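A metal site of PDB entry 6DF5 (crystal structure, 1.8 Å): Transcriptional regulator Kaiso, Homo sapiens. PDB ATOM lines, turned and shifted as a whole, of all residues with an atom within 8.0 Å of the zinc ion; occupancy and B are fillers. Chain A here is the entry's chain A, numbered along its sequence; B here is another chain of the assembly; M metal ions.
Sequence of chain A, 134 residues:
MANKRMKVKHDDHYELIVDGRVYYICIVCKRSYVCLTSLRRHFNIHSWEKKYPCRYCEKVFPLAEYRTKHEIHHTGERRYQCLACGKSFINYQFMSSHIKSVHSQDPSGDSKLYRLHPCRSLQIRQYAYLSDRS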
ATOM      1  N   ASP A  12      -7.951  21.656 -12.671  1.00  0.00           N
ATOM      2  CA  ASP A  12      -8.689  22.584 -13.535  1.00  0.00           C
ATOM      3  C   ASP A  12      -8.628  22.178 -15.017  1.00  0.00           C
ATOM      4  O   ASP A  12      -9.622  22.269 -15.752  1.00  0.00           O
ATOM      5  CB  ASP A  12      -8.153  23.995 -13.343  1.00  0.00           C
ATOM      6  CG  ASP A  12      -8.569  24.913 -14.480  1.00  0.00           C
ATOM      7  OD1 ASP A  12      -9.784  24.965 -14.795  1.00  0.00           O
ATOM      8  OD2 ASP A  12      -7.682  25.576 -15.059  1.00  0.00           O
ATOM      9  N   ILE A  25      -6.342  20.103 -21.875  1.00  0.00           N
ATOM     10  CA  ILE A  25      -7.565  19.330 -21.882  1.00  0.00           C
ATOM     11  C   ILE A  25      -8.481  19.773 -20.761  1.00  0.00           C
ATOM     12  O   ILE A  25      -8.078  19.791 -19.595  1.00  0.00           O
ATOM     13  CB  ILE A  25      -7.240  17.804 -21.710  1.00  0.00           C
ATOM     14  CG1 ILE A  25      -6.114  17.378 -22.653  1.00  0.00           C
ATOM     15  CG2 ILE A  25      -8.499  16.944 -21.885  1.00  0.00           C
ATOM     16  CD1 ILE A  25      -6.371  17.741 -24.113  1.00  0.00           C
ATOM     17  N   CYS A  26      -9.719  20.143 -21.098  1.00  0.00           N
ATOM     18  CA  CYS A  26     -10.708  20.481 -20.093  1.00  0.00           C
ATOM     19  C   CYS A  26     -11.029  19.276 -19.211  1.00  0.00           C
ATOM     20  O   CYS A  26     -11.215  18.180 -19.721  1.00  0.00           O
ATOM     21  CB  CYS A  26     -11.999  20.959 -20.743  1.00  0.00           C
ATOM     22  SG  CYS A  26     -13.254  21.350 -19.518  1.00  0.00           S
ATOM     23  N   ILE A  27     -11.121  19.484 -17.902  1.00  0.00           N
ATOM     24  CA  ILE A  27     -11.375  18.352 -16.991  1.00  0.00           C
ATOM     25  C   ILE A  27     -12.806  17.837 -17.162  1.00  0.00           C
ATOM     26  O   ILE A  27     -13.055  16.638 -17.140  1.00  0.00           O
ATOM     27  CB  ILE A  27     -11.157  18.720 -15.514  1.00  0.00           C
ATOM     28  CG1 ILE A  27      -9.680  18.984 -15.253  1.00  0.00           C
ATOM     29  CG2 ILE A  27     -11.632  17.598 -14.601  1.00  0.00           C
ATOM     30  CD1 ILE A  27      -9.285  18.983 -13.779  1.00  0.00           C
ATOM     31  N   VAL A  28     -13.729  18.769 -17.404  1.00  0.00           N
ATOM     32  CA  VAL A  28     -15.145  18.420 -17.397  1.00  0.00           C
ATOM     33  C   VAL A  28     -15.617  17.755 -18.698  1.00  0.00           C
ATOM     34  O   VAL A  28     -16.218  16.672 -18.650  1.00  0.00           O
ATOM     35  CB  VAL A  28     -16.001  19.667 -17.124  1.00  0.00           C
ATOM     36  CG1 VAL A  28     -17.453  19.406 -17.448  1.00  0.00           C
ATOM     37  CG2 VAL A  28     -15.827  20.104 -15.671  1.00  0.00           C
ATOM     38  N   CYS A  29     -15.358  18.380 -19.844  1.00  0.00           N
ATOM     39  CA  CYS A  29     -15.838  17.857 -21.119  1.00  0.00           C
ATOM     40  C   CYS A  29     -14.744  17.224 -21.989  1.00  0.00           C
ATOM     41  O   CYS A  29     -15.024  16.710 -23.075  1.00  0.00           O
ATOM     42  CB  CYS A  29     -16.540  18.962 -21.925  1.00  0.00           C
ATOM     43  SG  CYS A  29     -15.470  20.322 -22.416  1.00  0.00           S
ATOM     44  N   LYS A  30     -13.492  17.258 -21.506  1.00  0.00           N
ATOM     45  CA  LYS A  30     -12.339  16.726 -22.240  1.00  0.00           C
ATOM     46  C   LYS A  30     -12.013  17.395 -23.597  1.00  0.00           C
ATOM     47  O   LYS A  30     -11.339  16.795 -24.428  1.00  0.00           O
ATOM     48  CB  LYS A  30     -12.498  15.203 -22.469  1.00  0.00           C
ATOM     49  CG  LYS A  30     -12.966  14.407 -21.246  1.00  0.00           C
ATOM     50  CD  LYS A  30     -14.067  13.407 -21.611  1.00  0.00           C
ATOM     51  CE  LYS A  30     -14.980  13.103 -20.418  1.00  0.00           C
ATOM     52  NZ  LYS A  30     -15.914  11.961 -20.689  1.00  0.00           N
ATOM     53  N   ARG A  31     -12.465  18.628 -23.825  1.00  0.00           N
ATOM     54  CA  ARG A  31     -12.091  19.345 -25.051  1.00  0.00           C
ATOM     55  C   ARG A  31     -10.621  19.761 -25.010  1.00  0.00           C
ATOM     56  O   ARG A  31     -10.113  20.138 -23.949  1.00  0.00           O
ATOM     57  CB  ARG A  31     -12.965  20.590 -25.282  1.00  0.00           C
ATOM     58  CG  ARG A  31     -14.353  20.237 -25.762  1.00  0.00           C
ATOM     59  CD  ARG A  31     -15.269  21.461 -25.906  1.00  0.00           C
ATOM     60  NE  ARG A  31     -16.644  21.006 -26.074  1.00  0.00           N
ATOM     61  CZ  ARG A  31     -17.311  21.034 -27.217  1.00  0.00           C
ATOM     62  NH1 ARG A  31     -16.759  21.548 -28.312  1.00  0.00           N
ATOM     63  NH2 ARG A  31     -18.559  20.570 -27.255  1.00  0.00           N
ATOM     64  N   SER A  32      -9.949  19.684 -26.155  1.00  0.00           N
ATOM     65  CA  SER A  32      -8.531  20.023 -26.244  1.00  0.00           C
ATOM     66  C   SER A  32      -8.299  21.424 -26.810  1.00  0.00           C
ATOM     67  O   SER A  32      -8.992  21.883 -27.716  1.00  0.00           O
ATOM     68  CB  SER A  32      -7.770  18.988 -27.085  1.00  0.00           C
ATOM     69  OG  SER A  32      -8.263  18.924 -28.421  1.00  0.00           O
ATOM     70  N   TYR A  33      -7.293  22.094 -26.259  1.00  0.00           N
ATOM     71  CA  TYR A  33      -6.966  23.447 -26.655  1.00  0.00           C
ATOM     72  C   TYR A  33      -5.456  23.589 -26.806  1.00  0.00           C
ATOM     73  O   TYR A  33      -4.675  22.944 -26.084  1.00  0.00           O
ATOM     74  CB  TYR A  33      -7.511  24.431 -25.623  1.00  0.00           C
ATOM     75  CG  TYR A  33      -9.010  24.324 -25.521  1.00  0.00           C
ATOM     76  CD1 TYR A  33      -9.831  25.055 -26.386  1.00  0.00           C
ATOM     77  CD2 TYR A  33      -9.616  23.471 -24.603  1.00  0.00           C
ATOM     78  CE1 TYR A  33     -11.184  24.953 -26.338  1.00  0.00           C
ATOM     79  CE2 TYR A  33     -10.998  23.370 -24.536  1.00  0.00           C
ATOM     80  CZ  TYR A  33     -11.777  24.136 -25.419  1.00  0.00           C
ATOM     81  OH  TYR A  33     -13.145  24.043 -25.385  1.00  0.00           O
ATOM     82  N   LEU A  39      -8.596  27.501 -23.197  1.00  0.00           N
ATOM     83  CA  LEU A  39      -9.101  26.581 -22.187  1.00  0.00           C
ATOM     84  C   LEU A  39      -9.819  27.369 -21.096  1.00  0.00           C
ATOM     85  O   LEU A  39     -10.896  26.981 -20.654  1.00  0.00           O
ATOM     86  CB  LEU A  39      -7.954  25.742 -21.581  1.00  0.00           C
ATOM     87  CG  LEU A  39      -8.248  24.793 -20.418  1.00  0.00           C
ATOM     88  CD1 LEU A  39      -8.263  25.506 -19.051  1.00  0.00           C
ATOM     89  CD2 LEU A  39      -9.520  23.969 -20.645  1.00  0.00           C
ATOM     90  N   HIS A  42     -13.050  29.028 -22.411  1.00  0.00           N
ATOM     91  CA  HIS A  42     -14.012  27.943 -22.525  1.00  0.00           C
ATOM     92  C   HIS A  42     -14.616  27.503 -21.168  1.00  0.00           C
ATOM     93  O   HIS A  42     -15.814  27.221 -21.066  1.00  0.00           O
ATOM     94  CB  HIS A  42     -13.364  26.724 -23.176  1.00  0.00           C
ATOM     95  CG  HIS A  42     -14.109  25.455 -22.904  1.00  0.00           C
ATOM     96  ND1 HIS A  42     -15.231  25.084 -23.611  1.00  0.00           N
ATOM     97  CD2 HIS A  42     -13.912  24.490 -21.975  1.00  0.00           C
ATOM     98  CE1 HIS A  42     -15.684  23.936 -23.139  1.00  0.00           C
ATOM     99  NE2 HIS A  42     -14.908  23.561 -22.150  1.00  0.00           N
ATOM    100  N   PHE A  43     -13.793  27.435 -20.141  1.00  0.00           N
ATOM    101  CA  PHE A  43     -14.226  26.796 -18.900  1.00  0.00           C
ATOM    102  C   PHE A  43     -15.344  27.546 -18.179  1.00  0.00           C
ATOM    103  O   PHE A  43     -16.052  26.957 -17.366  1.00  0.00           O
ATOM    104  CB  PHE A  43     -13.036  26.610 -17.963  1.00  0.00           C
ATOM    105  CG  PHE A  43     -13.261  25.578 -16.895  1.00  0.00           C
ATOM    106  CD1 PHE A  43     -13.224  24.229 -17.210  1.00  0.00           C
ATOM    107  CD2 PHE A  43     -13.518  25.948 -15.588  1.00  0.00           C
ATOM    108  CE1 PHE A  43     -13.431  23.272 -16.232  1.00  0.00           C
ATOM    109  CE2 PHE A  43     -13.730  24.995 -14.603  1.00  0.00           C
ATOM    110  CZ  PHE A  43     -13.684  23.655 -14.929  1.00  0.00           C
ATOM    111  N   ASN A  44     -15.526  28.828 -18.486  1.00  0.00           N
ATOM    112  CA  ASN A  44     -16.597  29.596 -17.860  1.00  0.00           C
ATOM    113  C   ASN A  44     -17.967  28.975 -18.132  1.00  0.00           C
ATOM    114  O   ASN A  44     -18.890  29.133 -17.340  1.00  0.00           O
ATOM    115  CB  ASN A  44     -16.584  31.034 -18.358  1.00  0.00           C
ATOM    116  CG  ASN A  44     -17.238  31.982 -17.385  1.00  0.00           C
ATOM    117  OD1 ASN A  44     -17.005  31.907 -16.172  1.00  0.00           O
ATOM    118  ND2 ASN A  44     -18.089  32.885 -17.899  1.00  0.00           N
ATOM    119  N   ILE A  45     -18.077  28.295 -19.274  1.00  0.00           N
ATOM    120  CA  ILE A  45     -19.283  27.549 -19.652  1.00  0.00           C
ATOM    121  C   ILE A  45     -19.650  26.509 -18.589  1.00  0.00           C
ATOM    122  O   ILE A  45     -20.829  26.211 -18.365  1.00  0.00           O
ATOM    123  CB  ILE A  45     -19.079  26.853 -21.018  1.00  0.00           C
ATOM    124  CG1 ILE A  45     -18.939  27.869 -22.153  1.00  0.00           C
ATOM    125  CG2 ILE A  45     -20.192  25.851 -21.326  1.00  0.00           C
ATOM    126  CD1 ILE A  45     -18.471  27.254 -23.453  1.00  0.00           C
ATOM    127  N   HIS A  46     -18.637  25.945 -17.934  1.00  0.00           N
ATOM    128  CA  HIS A  46     -18.850  24.969 -16.874  1.00  0.00           C
ATOM    129  C   HIS A  46     -19.049  25.624 -15.511  1.00  0.00           C
ATOM    130  O   HIS A  46     -19.892  25.197 -14.720  1.00  0.00           O
ATOM    131  CB  HIS A  46     -17.680  23.998 -16.821  1.00  0.00           C
ATOM    132  CG  HIS A  46     -17.499  23.191 -18.069  1.00  0.00           C
ATOM    133  ND1 HIS A  46     -18.542  22.522 -18.680  1.00  0.00           N
ATOM    134  CD2 HIS A  46     -16.401  22.934 -18.821  1.00  0.00           C
ATOM    135  CE1 HIS A  46     -18.089  21.889 -19.753  1.00  0.00           C
ATOM    136  NE2 HIS A  46     -16.788  22.114 -19.854  1.00  0.00           N
ATOM    137  P    DT B   8     -13.940  24.669 -28.828  1.00  0.00           P
ATOM    138  OP1  DT B   8     -13.628  23.208 -28.961  1.00  0.00           O
ATOM    139  OP2  DT B   8     -14.300  25.190 -27.492  1.00  0.00           O
ATOM    140  O5'  DT B   8     -12.674  25.466 -29.351  1.00  0.00           O
ATOM    141  C5'  DT B   8     -12.045  25.056 -30.570  1.00  0.00           C
ATOM    142  C4'  DT B   8     -11.100  26.132 -31.056  1.00  0.00           C
ATOM    143  O4'  DT B   8     -11.860  27.306 -31.500  1.00  0.00           O
ATOM    144  C3'  DT B   8     -10.113  26.651 -30.010  1.00  0.00           C
ATOM    145  O3'  DT B   8      -8.852  26.810 -30.647  1.00  0.00           O
ATOM    146  C2'  DT B   8     -10.715  28.017 -29.635  1.00  0.00           C
ATOM    147  C1'  DT B   8     -11.233  28.450 -30.993  1.00  0.00           C
ATOM    148  N1   DT B   8     -12.210  29.581 -31.025  1.00  0.00           N
ATOM    149  C2   DT B   8     -12.275  30.344 -32.168  1.00  0.00           C
ATOM    150  O2   DT B   8     -11.529  30.171 -33.120  1.00  0.00           O
ATOM    151  N3   DT B   8     -13.206  31.355 -32.137  1.00  0.00           N
ATOM    152  C4   DT B   8     -14.085  31.639 -31.116  1.00  0.00           C
ATOM    153  O4   DT B   8     -14.897  32.571 -31.191  1.00  0.00           O
ATOM    154  C5   DT B   8     -13.991  30.795 -29.954  1.00  0.00           C
ATOM    155  C7   DT B   8     -14.900  31.039 -28.792  1.00  0.00           C
ATOM    156  C6   DT B   8     -13.067  29.802 -29.960  1.00  0.00           C
HETATM  157 ZN    ZN M   1     -15.084  21.861 -20.908  1.00  0.00          ZN
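A ring nitrogen (ND1) of His 42 lies within hydrogen-bond range of the side-chain hydroxyl (OH) of Tyr 33, at 2.9 Å.
SG of Cys 29 lies close to N of Arg 31, at 3.7 Å.
The side-chain sulfur of Cys 26 lies close to the backbone NH of Val 28, 3.4 Å away.
N of Cys 26 lies within hydrogen-bond range of O of Arg 31, at 2.9 Å.
Within 4 Å of the zinc ion: Cys 26, Cys 29, His 42 and His 46.
Along chain A the residues within 4 Å of the zinc ion span positions 26 to 46.
The nearest printed residue that does not touch the zinc ion is Val 28 (4.5 Å).
The zinc ion is bound by a ring nitrogen (NE2) of His 46 (2.0 Å), a ring nitrogen (NE2) of His 42 (2.1 Å), the side-chain sulfur of Cys 29 (2.2 Å) and the side-chain sulfur of Cys 26 (2.4 Å).
The zinc ion has four donor atoms within binding distance.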
